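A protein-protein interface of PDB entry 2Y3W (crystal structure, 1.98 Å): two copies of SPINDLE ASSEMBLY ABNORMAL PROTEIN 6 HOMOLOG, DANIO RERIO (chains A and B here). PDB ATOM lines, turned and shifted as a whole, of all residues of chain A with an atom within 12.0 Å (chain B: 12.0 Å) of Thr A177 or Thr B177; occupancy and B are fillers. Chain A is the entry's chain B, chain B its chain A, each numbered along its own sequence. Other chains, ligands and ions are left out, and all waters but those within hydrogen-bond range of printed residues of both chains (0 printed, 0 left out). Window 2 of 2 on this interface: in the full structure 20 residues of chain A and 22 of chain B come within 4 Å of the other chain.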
ATOM      1  N   GLN A 168      -9.827  28.991  -8.751  1.00  0.00           N
ATOM      2  CA  GLN A 168     -10.487  28.070  -7.832  1.00  0.00           C
ATOM      3  C   GLN A 168     -11.405  27.110  -8.581  1.00  0.00           C
ATOM      4  O   GLN A 168     -11.508  25.939  -8.228  1.00  0.00           O
ATOM      5  CB  GLN A 168     -11.283  28.833  -6.775  1.00  0.00           C
ATOM      6  CG  GLN A 168     -10.425  29.595  -5.783  1.00  0.00           C
ATOM      7  CD  GLN A 168     -11.255  30.478  -4.871  1.00  0.00           C
ATOM      8  OE1 GLN A 168     -12.456  30.653  -5.086  1.00  0.00           O
ATOM      9  NE2 GLN A 168     -10.618  31.040  -3.850  1.00  0.00           N
ATOM     10  N   GLN A 169     -12.076  27.614  -9.611  1.00  0.00           N
ATOM     11  CA  GLN A 169     -12.917  26.772 -10.449  1.00  0.00           C
ATOM     12  C   GLN A 169     -12.063  25.735 -11.171  1.00  0.00           C
ATOM     13  O   GLN A 169     -12.399  24.548 -11.197  1.00  0.00           O
ATOM     14  CB  GLN A 169     -13.698  27.627 -11.454  1.00  0.00           C
ATOM     15  CG  GLN A 169     -14.717  28.548 -10.804  1.00  0.00           C
ATOM     16  CD  GLN A 169     -15.271  29.589 -11.761  1.00  0.00           C
ATOM     17  OE1 GLN A 169     -14.883  29.648 -12.931  1.00  0.00           O
ATOM     18  NE2 GLN A 169     -16.182  30.422 -11.264  1.00  0.00           N
ATOM     19  N   LEU A 170     -10.953  26.185 -11.749  1.00  0.00           N
ATOM     20  CA  LEU A 170     -10.032  25.279 -12.424  1.00  0.00           C
ATOM     21  C   LEU A 170      -9.494  24.205 -11.480  1.00  0.00           C
ATOM     22  O   LEU A 170      -9.280  23.060 -11.886  1.00  0.00           O
ATOM     23  CB  LEU A 170      -8.866  26.049 -13.039  1.00  0.00           C
ATOM     24  CG  LEU A 170      -9.142  26.861 -14.301  1.00  0.00           C
ATOM     25  CD1 LEU A 170      -7.908  27.653 -14.698  1.00  0.00           C
ATOM     26  CD2 LEU A 170      -9.574  25.939 -15.426  1.00  0.00           C
ATOM     27  N   GLN A 171      -9.265  24.579 -10.227  1.00  0.00           N
ATOM     28  CA  GLN A 171      -8.776  23.623  -9.242  1.00  0.00           C
ATOM     29  C   GLN A 171      -9.843  22.590  -8.915  1.00  0.00           C
ATOM     30  O   GLN A 171      -9.545  21.401  -8.801  1.00  0.00           O
ATOM     31  CB  GLN A 171      -8.284  24.334  -7.977  1.00  0.00           C
ATOM     32  CG  GLN A 171      -6.836  24.819  -8.079  1.00  0.00           C
ATOM     33  CD  GLN A 171      -6.516  25.913  -7.079  1.00  0.00           C
ATOM     34  OE1 GLN A 171      -7.411  26.442  -6.417  1.00  0.00           O
ATOM     35  NE2 GLN A 171      -5.235  26.266  -6.972  1.00  0.00           N
ATOM     36  N   GLN A 172     -11.084  23.047  -8.769  1.00  0.00           N
ATOM     37  CA  GLN A 172     -12.216  22.145  -8.554  1.00  0.00           C
ATOM     38  C   GLN A 172     -12.359  21.167  -9.715  1.00  0.00           C
ATOM     39  O   GLN A 172     -12.570  19.974  -9.507  1.00  0.00           O
ATOM     40  CB  GLN A 172     -13.524  22.922  -8.393  1.00  0.00           C
ATOM     41  CG  GLN A 172     -13.624  23.778  -7.140  1.00  0.00           C
ATOM     42  CD  GLN A 172     -15.033  24.303  -6.914  1.00  0.00           C
ATOM     43  OE1 GLN A 172     -16.017  23.655  -7.280  1.00  0.00           O
ATOM     44  NE2 GLN A 172     -15.138  25.486  -6.314  1.00  0.00           N
ATOM     45  N   LYS A 173     -12.250  21.676 -10.938  1.00  0.00           N
ATOM     46  CA  LYS A 173     -12.385  20.828 -12.115  1.00  0.00           C
ATOM     47  C   LYS A 173     -11.266  19.798 -12.159  1.00  0.00           C
ATOM     48  O   LYS A 173     -11.498  18.626 -12.454  1.00  0.00           O
ATOM     49  CB  LYS A 173     -12.388  21.657 -13.398  1.00  0.00           C
ATOM     50  CG  LYS A 173     -12.640  20.824 -14.643  1.00  0.00           C
ATOM     51  CD  LYS A 173     -12.684  21.671 -15.898  1.00  0.00           C
ATOM     52  CE  LYS A 173     -12.856  20.799 -17.133  1.00  0.00           C
ATOM     53  NZ  LYS A 173     -12.513  21.523 -18.389  1.00  0.00           N
ATOM     54  N   LEU A 174     -10.052  20.244 -11.865  1.00  0.00           N
ATOM     55  CA  LEU A 174      -8.904  19.351 -11.812  1.00  0.00           C
ATOM     56  C   LEU A 174      -9.133  18.243 -10.783  1.00  0.00           C
ATOM     57  O   LEU A 174      -8.837  17.073 -11.027  1.00  0.00           O
ATOM     58  CB  LEU A 174      -7.642  20.138 -11.460  1.00  0.00           C
ATOM     59  CG  LEU A 174      -6.324  19.367 -11.421  1.00  0.00           C
ATOM     60  CD1 LEU A 174      -6.052  18.705 -12.765  1.00  0.00           C
ATOM     61  CD2 LEU A 174      -5.187  20.300 -11.034  1.00  0.00           C
ATOM     62  N   ARG A 175      -9.670  18.623  -9.631  1.00  0.00           N
ATOM     63  CA  ARG A 175      -9.918  17.668  -8.558  1.00  0.00           C
ATOM     64  C   ARG A 175     -10.897  16.597  -9.025  1.00  0.00           C
ATOM     65  O   ARG A 175     -10.650  15.402  -8.865  1.00  0.00           O
ATOM     66  CB  ARG A 175     -10.458  18.384  -7.319  1.00  0.00           C
ATOM     67  CG  ARG A 175     -10.674  17.481  -6.112  1.00  0.00           C
ATOM     68  CD  ARG A 175     -11.212  18.267  -4.920  1.00  0.00           C
ATOM     69  NE  ARG A 175     -12.476  18.937  -5.224  1.00  0.00           N
ATOM     70  CZ  ARG A 175     -13.673  18.375  -5.086  1.00  0.00           C
ATOM     71  NH1 ARG A 175     -13.778  17.129  -4.645  1.00  0.00           N
ATOM     72  NH2 ARG A 175     -14.768  19.061  -5.389  1.00  0.00           N
ATOM     73  N   LYS A 176     -12.004  17.036  -9.613  1.00  0.00           N
ATOM     74  CA  LYS A 176     -13.024  16.122 -10.112  1.00  0.00           C
ATOM     75  C   LYS A 176     -12.498  15.261 -11.257  1.00  0.00           C
ATOM     76  O   LYS A 176     -12.736  14.055 -11.296  1.00  0.00           O
ATOM     77  CB  LYS A 176     -14.262  16.906 -10.546  1.00  0.00           C
ATOM     78  CG  LYS A 176     -14.947  17.625  -9.395  1.00  0.00           C
ATOM     79  CD  LYS A 176     -15.877  18.726  -9.880  1.00  0.00           C
ATOM     80  CE  LYS A 176     -16.419  19.533  -8.708  1.00  0.00           C
ATOM     81  NZ  LYS A 176     -17.151  20.752  -9.150  1.00  0.00           N
ATOM     82  N   THR A 177     -11.776  15.880 -12.183  1.00  0.00           N
ATOM     83  CA  THR A 177     -11.192  15.156 -13.307  1.00  0.00           C
ATOM     84  C   THR A 177     -10.243  14.056 -12.838  1.00  0.00           C
ATOM     85  O   THR A 177     -10.259  12.943 -13.366  1.00  0.00           O
ATOM     86  CB  THR A 177     -10.430  16.101 -14.267  1.00  0.00           C
ATOM     87  OG1 THR A 177     -11.367  16.881 -15.021  1.00  0.00           O
ATOM     88  CG2 THR A 177      -9.566  15.303 -15.231  1.00  0.00           C
ATOM     89  N   GLU A 178      -9.426  14.369 -11.837  1.00  0.00           N
ATOM     90  CA  GLU A 178      -8.381  13.452 -11.388  1.00  0.00           C
ATOM     91  C   GLU A 178      -8.909  12.192 -10.705  1.00  0.00           C
ATOM     92  O   GLU A 178      -8.253  11.149 -10.725  1.00  0.00           O
ATOM     93  CB  GLU A 178      -7.375  14.170 -10.483  1.00  0.00           C
ATOM     94  CG  GLU A 178      -6.327  14.962 -11.248  1.00  0.00           C
ATOM     95  CD  GLU A 178      -5.240  15.516 -10.348  1.00  0.00           C
ATOM     96  OE1 GLU A 178      -5.551  15.872  -9.192  1.00  0.00           O
ATOM     97  OE2 GLU A 178      -4.074  15.587 -10.800  1.00  0.00           O
ATOM     98  N   GLU A 179     -10.088  12.290 -10.103  1.00  0.00           N
ATOM     99  CA  GLU A 179     -10.708  11.129  -9.479  1.00  0.00           C
ATOM    100  C   GLU A 179     -11.355  10.249 -10.541  1.00  0.00           C
ATOM    101  O   GLU A 179     -12.111   9.331 -10.226  1.00  0.00           O
ATOM    102  CB  GLU A 179     -11.745  11.564  -8.448  1.00  0.00           C
ATOM    103  CG  GLU A 179     -11.172  12.393  -7.311  1.00  0.00           C
ATOM    104  CD  GLU A 179     -12.236  12.837  -6.328  1.00  0.00           C
ATOM    105  OE1 GLU A 179     -13.432  12.608  -6.607  1.00  0.00           O
ATOM    106  OE2 GLU A 179     -11.878  13.415  -5.279  1.00  0.00           O
ATOM    107  N   ASP A 180     -11.051  10.540 -11.801  1.00  0.00           N
ATOM    108  CA  ASP A 180     -11.625   9.811 -12.925  1.00  0.00           C
ATOM    109  C   ASP A 180     -10.538   9.267 -13.851  1.00  0.00           C
ATOM    110  O   ASP A 180      -9.696   8.469 -13.436  1.00  0.00           O
ATOM    111  CB  ASP A 180     -12.576  10.716 -13.713  1.00  0.00           C
ATOM    112  CG  ASP A 180     -13.658  11.325 -12.844  1.00  0.00           C
ATOM    113  OD1 ASP A 180     -13.820  10.877 -11.691  1.00  0.00           O
ATOM    114  OD2 ASP A 180     -14.354  12.247 -13.320  1.00  0.00           O
ATOM    115  N   LYS B 167      -2.591  30.616 -13.217  1.00  0.00           N
ATOM    116  CA  LYS B 167      -3.804  30.123 -13.855  1.00  0.00           C
ATOM    117  C   LYS B 167      -3.495  29.447 -15.183  1.00  0.00           C
ATOM    118  O   LYS B 167      -4.080  28.416 -15.522  1.00  0.00           O
ATOM    119  CB  LYS B 167      -4.801  31.257 -14.083  1.00  0.00           C
ATOM    120  CG  LYS B 167      -6.229  30.763 -14.293  1.00  0.00           C
ATOM    121  CD  LYS B 167      -7.162  31.869 -14.754  1.00  0.00           C
ATOM    122  CE  LYS B 167      -6.954  32.175 -16.225  1.00  0.00           C
ATOM    123  NZ  LYS B 167      -7.986  33.118 -16.740  1.00  0.00           N
ATOM    124  N   GLN B 168      -2.577  30.039 -15.937  1.00  0.00           N
ATOM    125  CA  GLN B 168      -2.195  29.497 -17.230  1.00  0.00           C
ATOM    126  C   GLN B 168      -1.553  28.129 -17.050  1.00  0.00           C
ATOM    127  O   GLN B 168      -1.895  27.180 -17.752  1.00  0.00           O
ATOM    128  CB  GLN B 168      -1.241  30.454 -17.946  1.00  0.00           C
ATOM    129  CG  GLN B 168      -0.765  29.981 -19.308  1.00  0.00           C
ATOM    130  CD  GLN B 168       0.159  30.980 -19.968  1.00  0.00           C
ATOM    131  OE1 GLN B 168       0.345  32.099 -19.473  1.00  0.00           O
ATOM    132  NE2 GLN B 168       0.751  30.583 -21.095  1.00  0.00           N
ATOM    133  N   GLN B 169      -0.638  28.024 -16.088  1.00  0.00           N
ATOM    134  CA  GLN B 169       0.018  26.751 -15.797  1.00  0.00           C
ATOM    135  C   GLN B 169      -0.983  25.686 -15.367  1.00  0.00           C
ATOM    136  O   GLN B 169      -0.864  24.518 -15.733  1.00  0.00           O
ATOM    137  CB  GLN B 169       1.107  26.942 -14.735  1.00  0.00           C
ATOM    138  CG  GLN B 169       2.311  27.710 -15.254  1.00  0.00           C
ATOM    139  CD  GLN B 169       3.107  28.383 -14.143  1.00  0.00           C
ATOM    140  OE1 GLN B 169       2.756  28.287 -12.971  1.00  0.00           O
ATOM    141  NE2 GLN B 169       4.178  29.074 -14.513  1.00  0.00           N
ATOM    142  N   LEU B 170      -1.981  26.099 -14.598  1.00  0.00           N
ATOM    143  CA  LEU B 170      -3.008  25.186 -14.141  1.00  0.00           C
ATOM    144  C   LEU B 170      -3.870  24.735 -15.316  1.00  0.00           C
ATOM    145  O   LEU B 170      -4.298  23.580 -15.374  1.00  0.00           O
ATOM    146  CB  LEU B 170      -3.864  25.843 -13.053  1.00  0.00           C
ATOM    147  CG  LEU B 170      -5.035  25.049 -12.481  1.00  0.00           C
ATOM    148  CD1 LEU B 170      -4.571  23.754 -11.836  1.00  0.00           C
ATOM    149  CD2 LEU B 170      -5.791  25.906 -11.487  1.00  0.00           C
ATOM    150  N   GLN B 171      -4.107  25.647 -16.257  1.00  0.00           N
ATOM    151  CA  GLN B 171      -4.866  25.324 -17.462  1.00  0.00           C
ATOM    152  C   GLN B 171      -4.121  24.301 -18.314  1.00  0.00           C
ATOM    153  O   GLN B 171      -4.696  23.312 -18.761  1.00  0.00           O
ATOM    154  CB  GLN B 171      -5.162  26.588 -18.275  1.00  0.00           C
ATOM    155  CG  GLN B 171      -6.364  27.381 -17.768  1.00  0.00           C
ATOM    156  CD  GLN B 171      -6.474  28.772 -18.377  1.00  0.00           C
ATOM    157  OE1 GLN B 171      -5.470  29.409 -18.702  1.00  0.00           O
ATOM    158  NE2 GLN B 171      -7.705  29.253 -18.527  1.00  0.00           N
ATOM    159  N   GLN B 172      -2.834  24.539 -18.530  1.00  0.00           N
ATOM    160  CA  GLN B 172      -2.019  23.623 -19.318  1.00  0.00           C
ATOM    161  C   GLN B 172      -1.989  22.244 -18.674  1.00  0.00           C
ATOM    162  O   GLN B 172      -1.995  21.222 -19.359  1.00  0.00           O
ATOM    163  CB  GLN B 172      -0.602  24.166 -19.482  1.00  0.00           C
ATOM    164  CG  GLN B 172       0.357  23.191 -20.145  1.00  0.00           C
ATOM    165  CD  GLN B 172       1.658  23.848 -20.563  1.00  0.00           C
ATOM    166  OE1 GLN B 172       1.761  25.074 -20.607  1.00  0.00           O
ATOM    167  NE2 GLN B 172       2.663  23.032 -20.875  1.00  0.00           N
ATOM    168  N   LYS B 173      -1.967  22.210 -17.349  1.00  0.00           N
ATOM    169  CA  LYS B 173      -1.957  20.929 -16.656  1.00  0.00           C
ATOM    170  C   LYS B 173      -3.281  20.197 -16.793  1.00  0.00           C
ATOM    171  O   LYS B 173      -3.309  18.990 -17.009  1.00  0.00           O
ATOM    172  CB  LYS B 173      -1.641  21.106 -15.180  1.00  0.00           C
ATOM    173  CG  LYS B 173      -1.861  19.841 -14.378  1.00  0.00           C
ATOM    174  CD  LYS B 173      -1.881  20.123 -12.890  1.00  0.00           C
ATOM    175  CE  LYS B 173      -1.940  18.822 -12.082  1.00  0.00           C
ATOM    176  NZ  LYS B 173      -1.580  18.959 -10.637  1.00  0.00           N
ATOM    177  N   LEU B 174      -4.378  20.926 -16.640  1.00  0.00           N
ATOM    178  CA  LEU B 174      -5.694  20.323 -16.758  1.00  0.00           C
ATOM    179  C   LEU B 174      -5.862  19.727 -18.150  1.00  0.00           C
ATOM    180  O   LEU B 174      -6.357  18.613 -18.297  1.00  0.00           O
ATOM    181  CB  LEU B 174      -6.794  21.348 -16.476  1.00  0.00           C
ATOM    182  CG  LEU B 174      -8.229  20.813 -16.527  1.00  0.00           C
ATOM    183  CD1 LEU B 174      -8.425  19.679 -15.539  1.00  0.00           C
ATOM    184  CD2 LEU B 174      -9.228  21.921 -16.261  1.00  0.00           C
ATOM    185  N   ARG B 175      -5.438  20.468 -19.170  1.00  0.00           N
ATOM    186  CA  ARG B 175      -5.502  19.978 -20.543  1.00  0.00           C
ATOM    187  C   ARG B 175      -4.828  18.620 -20.693  1.00  0.00           C
ATOM    188  O   ARG B 175      -5.422  17.676 -21.213  1.00  0.00           O
ATOM    189  CB  ARG B 175      -4.863  20.974 -21.505  1.00  0.00           C
ATOM    190  CG  ARG B 175      -5.773  22.113 -21.908  1.00  0.00           C
ATOM    191  CD  ARG B 175      -5.620  22.400 -23.387  1.00  0.00           C
ATOM    192  NE  ARG B 175      -5.668  21.164 -24.165  1.00  0.00           N
ATOM    193  CZ  ARG B 175      -5.721  21.112 -25.493  1.00  0.00           C
ATOM    194  NH1 ARG B 175      -5.738  22.232 -26.203  1.00  0.00           N
ATOM    195  NH2 ARG B 175      -5.760  19.939 -26.110  1.00  0.00           N
ATOM    196  N   LYS B 176      -3.582  18.528 -20.244  1.00  0.00           N
ATOM    197  CA  LYS B 176      -2.849  17.271 -20.311  1.00  0.00           C
ATOM    198  C   LYS B 176      -3.613  16.183 -19.566  1.00  0.00           C
ATOM    199  O   LYS B 176      -3.782  15.072 -20.069  1.00  0.00           O
ATOM    200  CB  LYS B 176      -1.443  17.429 -19.729  1.00  0.00           C
ATOM    201  CG  LYS B 176      -0.597  16.169 -19.813  1.00  0.00           C
ATOM    202  CD  LYS B 176       0.810  16.401 -19.283  1.00  0.00           C
ATOM    203  CE  LYS B 176       1.637  15.125 -19.356  1.00  0.00           C
ATOM    204  NZ  LYS B 176       3.027  15.321 -18.864  1.00  0.00           N
ATOM    205  N   THR B 177      -4.078  16.515 -18.366  1.00  0.00           N
ATOM    206  CA  THR B 177      -4.854  15.580 -17.561  1.00  0.00           C
ATOM    207  C   THR B 177      -6.125  15.174 -18.299  1.00  0.00           C
ATOM    208  O   THR B 177      -6.530  14.013 -18.272  1.00  0.00           O
ATOM    209  CB  THR B 177      -5.237  16.193 -16.201  1.00  0.00           C
ATOM    210  OG1 THR B 177      -4.058  16.651 -15.525  1.00  0.00           O
ATOM    211  CG2 THR B 177      -5.948  15.166 -15.332  1.00  0.00           C
ATOM    212  N   GLU B 178      -6.746  16.146 -18.958  1.00  0.00           N
ATOM    213  CA  GLU B 178      -7.973  15.920 -19.713  1.00  0.00           C
ATOM    214  C   GLU B 178      -7.760  14.886 -20.817  1.00  0.00           C
ATOM    215  O   GLU B 178      -8.605  14.019 -21.037  1.00  0.00           O
ATOM    216  CB  GLU B 178      -8.477  17.239 -20.309  1.00  0.00           C
ATOM    217  CG  GLU B 178      -9.774  17.125 -21.098  1.00  0.00           C
ATOM    218  CD  GLU B 178     -10.975  16.833 -20.215  1.00  0.00           C
ATOM    219  OE1 GLU B 178     -10.863  17.002 -18.981  1.00  0.00           O
ATOM    220  OE2 GLU B 178     -12.031  16.435 -20.754  1.00  0.00           O
ATOM    221  N   GLU B 179      -6.626  14.981 -21.504  1.00  0.00           N
ATOM    222  CA  GLU B 179      -6.300  14.057 -22.587  1.00  0.00           C
ATOM    223  C   GLU B 179      -6.162  12.614 -22.102  1.00  0.00           C
ATOM    224  O   GLU B 179      -6.125  12.349 -20.901  1.00  0.00           O
ATOM    225  CB  GLU B 179      -5.013  14.493 -23.287  1.00  0.00           C
ATOM    226  CG  GLU B 179      -5.098  15.849 -23.965  1.00  0.00           C
ATOM    227  CD  GLU B 179      -3.788  16.250 -24.618  1.00  0.00           C
ATOM    228  OE1 GLU B 179      -2.756  15.610 -24.320  1.00  0.00           O
ATOM    229  OE2 GLU B 179      -3.787  17.201 -25.432  1.00  0.00           O
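The side-chain hydroxyl (OG1) of Thr B177 sits at hydrogen-bond distance from the backbone carbonyl oxygen (O) of Lys B173.
OG1 of Thr A177 is in hydrogen-bond range of O of Lys A173, 3.1 Å away.
CD2 of Leu B170 touches CB of Leu A170, 3.4 Å away.
Leu A170 touches Gln B171 (CD1 to CG, 3.4 Å).
Gln A171 touches Leu B170 (CG to CD2, 3.7 Å).
CD of Lys A173 touches CD2 of Leu B174, 3.5 Å away.
Leu B170 touches Leu A174 (CD1 to CD2, 3.6 Å).
CD2 of Leu A174 touches CE of Lys B173, at 3.7 Å.
CA of Leu A174 touches CD1 of Leu B174, at 3.8 Å.
Leu A174 touches Thr B177 (CD1 to OG1, 3.98 Å).
CG2 of Thr A177 touches CG2 of Thr B177, at 3.6 Å.
Glu B178 touches Thr A177.
Of the printed residues of chain B, Thr A177 touches Thr B177 and Glu B178.
Thr B177 touches just these residues of chain A: Leu A174 (3.98 Å) and Thr A177 (3.6 Å).
Lys A173 touches one residue of chain B.
Leu A174 touches just these residues of chain B: Leu B170 (3.6 Å), Lys B173 (3.7 Å), Leu B174 (3.8 Å) and Thr B177 (3.98 Å).
No residue of chain B comes within 4 Å of Lys A176.
Glu A178 touches none of the printed residues of chain B.
No residue of chain B comes within 4 Å of Glu A179.
No residue of chain B comes within 4 Å of Asp A180.
Lys B173 touches just one residue of chain A: Leu A174.
Of chain A, only Lys A173 and Leu A174 come within 4 Å of Leu B174.
Lys B176 touches none of the printed residues of chain A.
No residue of chain A comes within 4 Å of Glu B179.
Printed residues of chain A within 4 Å of Leu B170: Leu A170, Gln A171 and Leu A174.
Of the printed residues of chain A, Glu B178 touches Thr A177 (3.99 Å).
Of the printed residues of chain B, Gln A171 touches Leu B170 (3.7 Å).
Printed residues of chain A within 4 Å of Gln B171: Leu A170.
Printed residues of chain B within 4 Å of Leu A170: Lys B167, Leu B170 and Gln B171.
Arg A175 touches none of the printed residues of chain B.
Gln A168 touches none of the printed residues of chain B.
The nearest printed residue of chain B that does not touch Thr A177 is Leu B174 (4.1 Å).
The nearest residue of chain A that does not touch Thr B177 is Glu A178 (4.1 Å).
Of the 13 printed residues of chain A, 5 touch a printed residue of chain B.
Hydrophobic or aromatic side chains of chain A within 4 Å of the printed part of chain B: Leu A170 and Leu A174.
Hydrophobic or aromatic side chains of chain B that line the printed part of chain A: Leu B170 and Leu B174.
Among the printed residues, no Asp or Glu carboxylate lies within 4 Å of a Lys or Arg side-chain nitrogen of the other chain.
Leu A170 touches its own counterpart, Leu B170.
Lys A173 touches Leu B174, and with the chains exchanged Leu A174 touches Lys B173.
Leu A174 touches Leu B170, but with the chains exchanged Leu A170 does not touch Leu B174 (4.1 Å).
Thr A177 touches Glu B178, but with the chains exchanged Glu A178 does not touch Thr B177 (4.1 Å).
12 positions are printed for both chains.
Of the 11 pairs that touch across the chains among the printed residues, 7 have their exchanged pair printed and touching as well.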
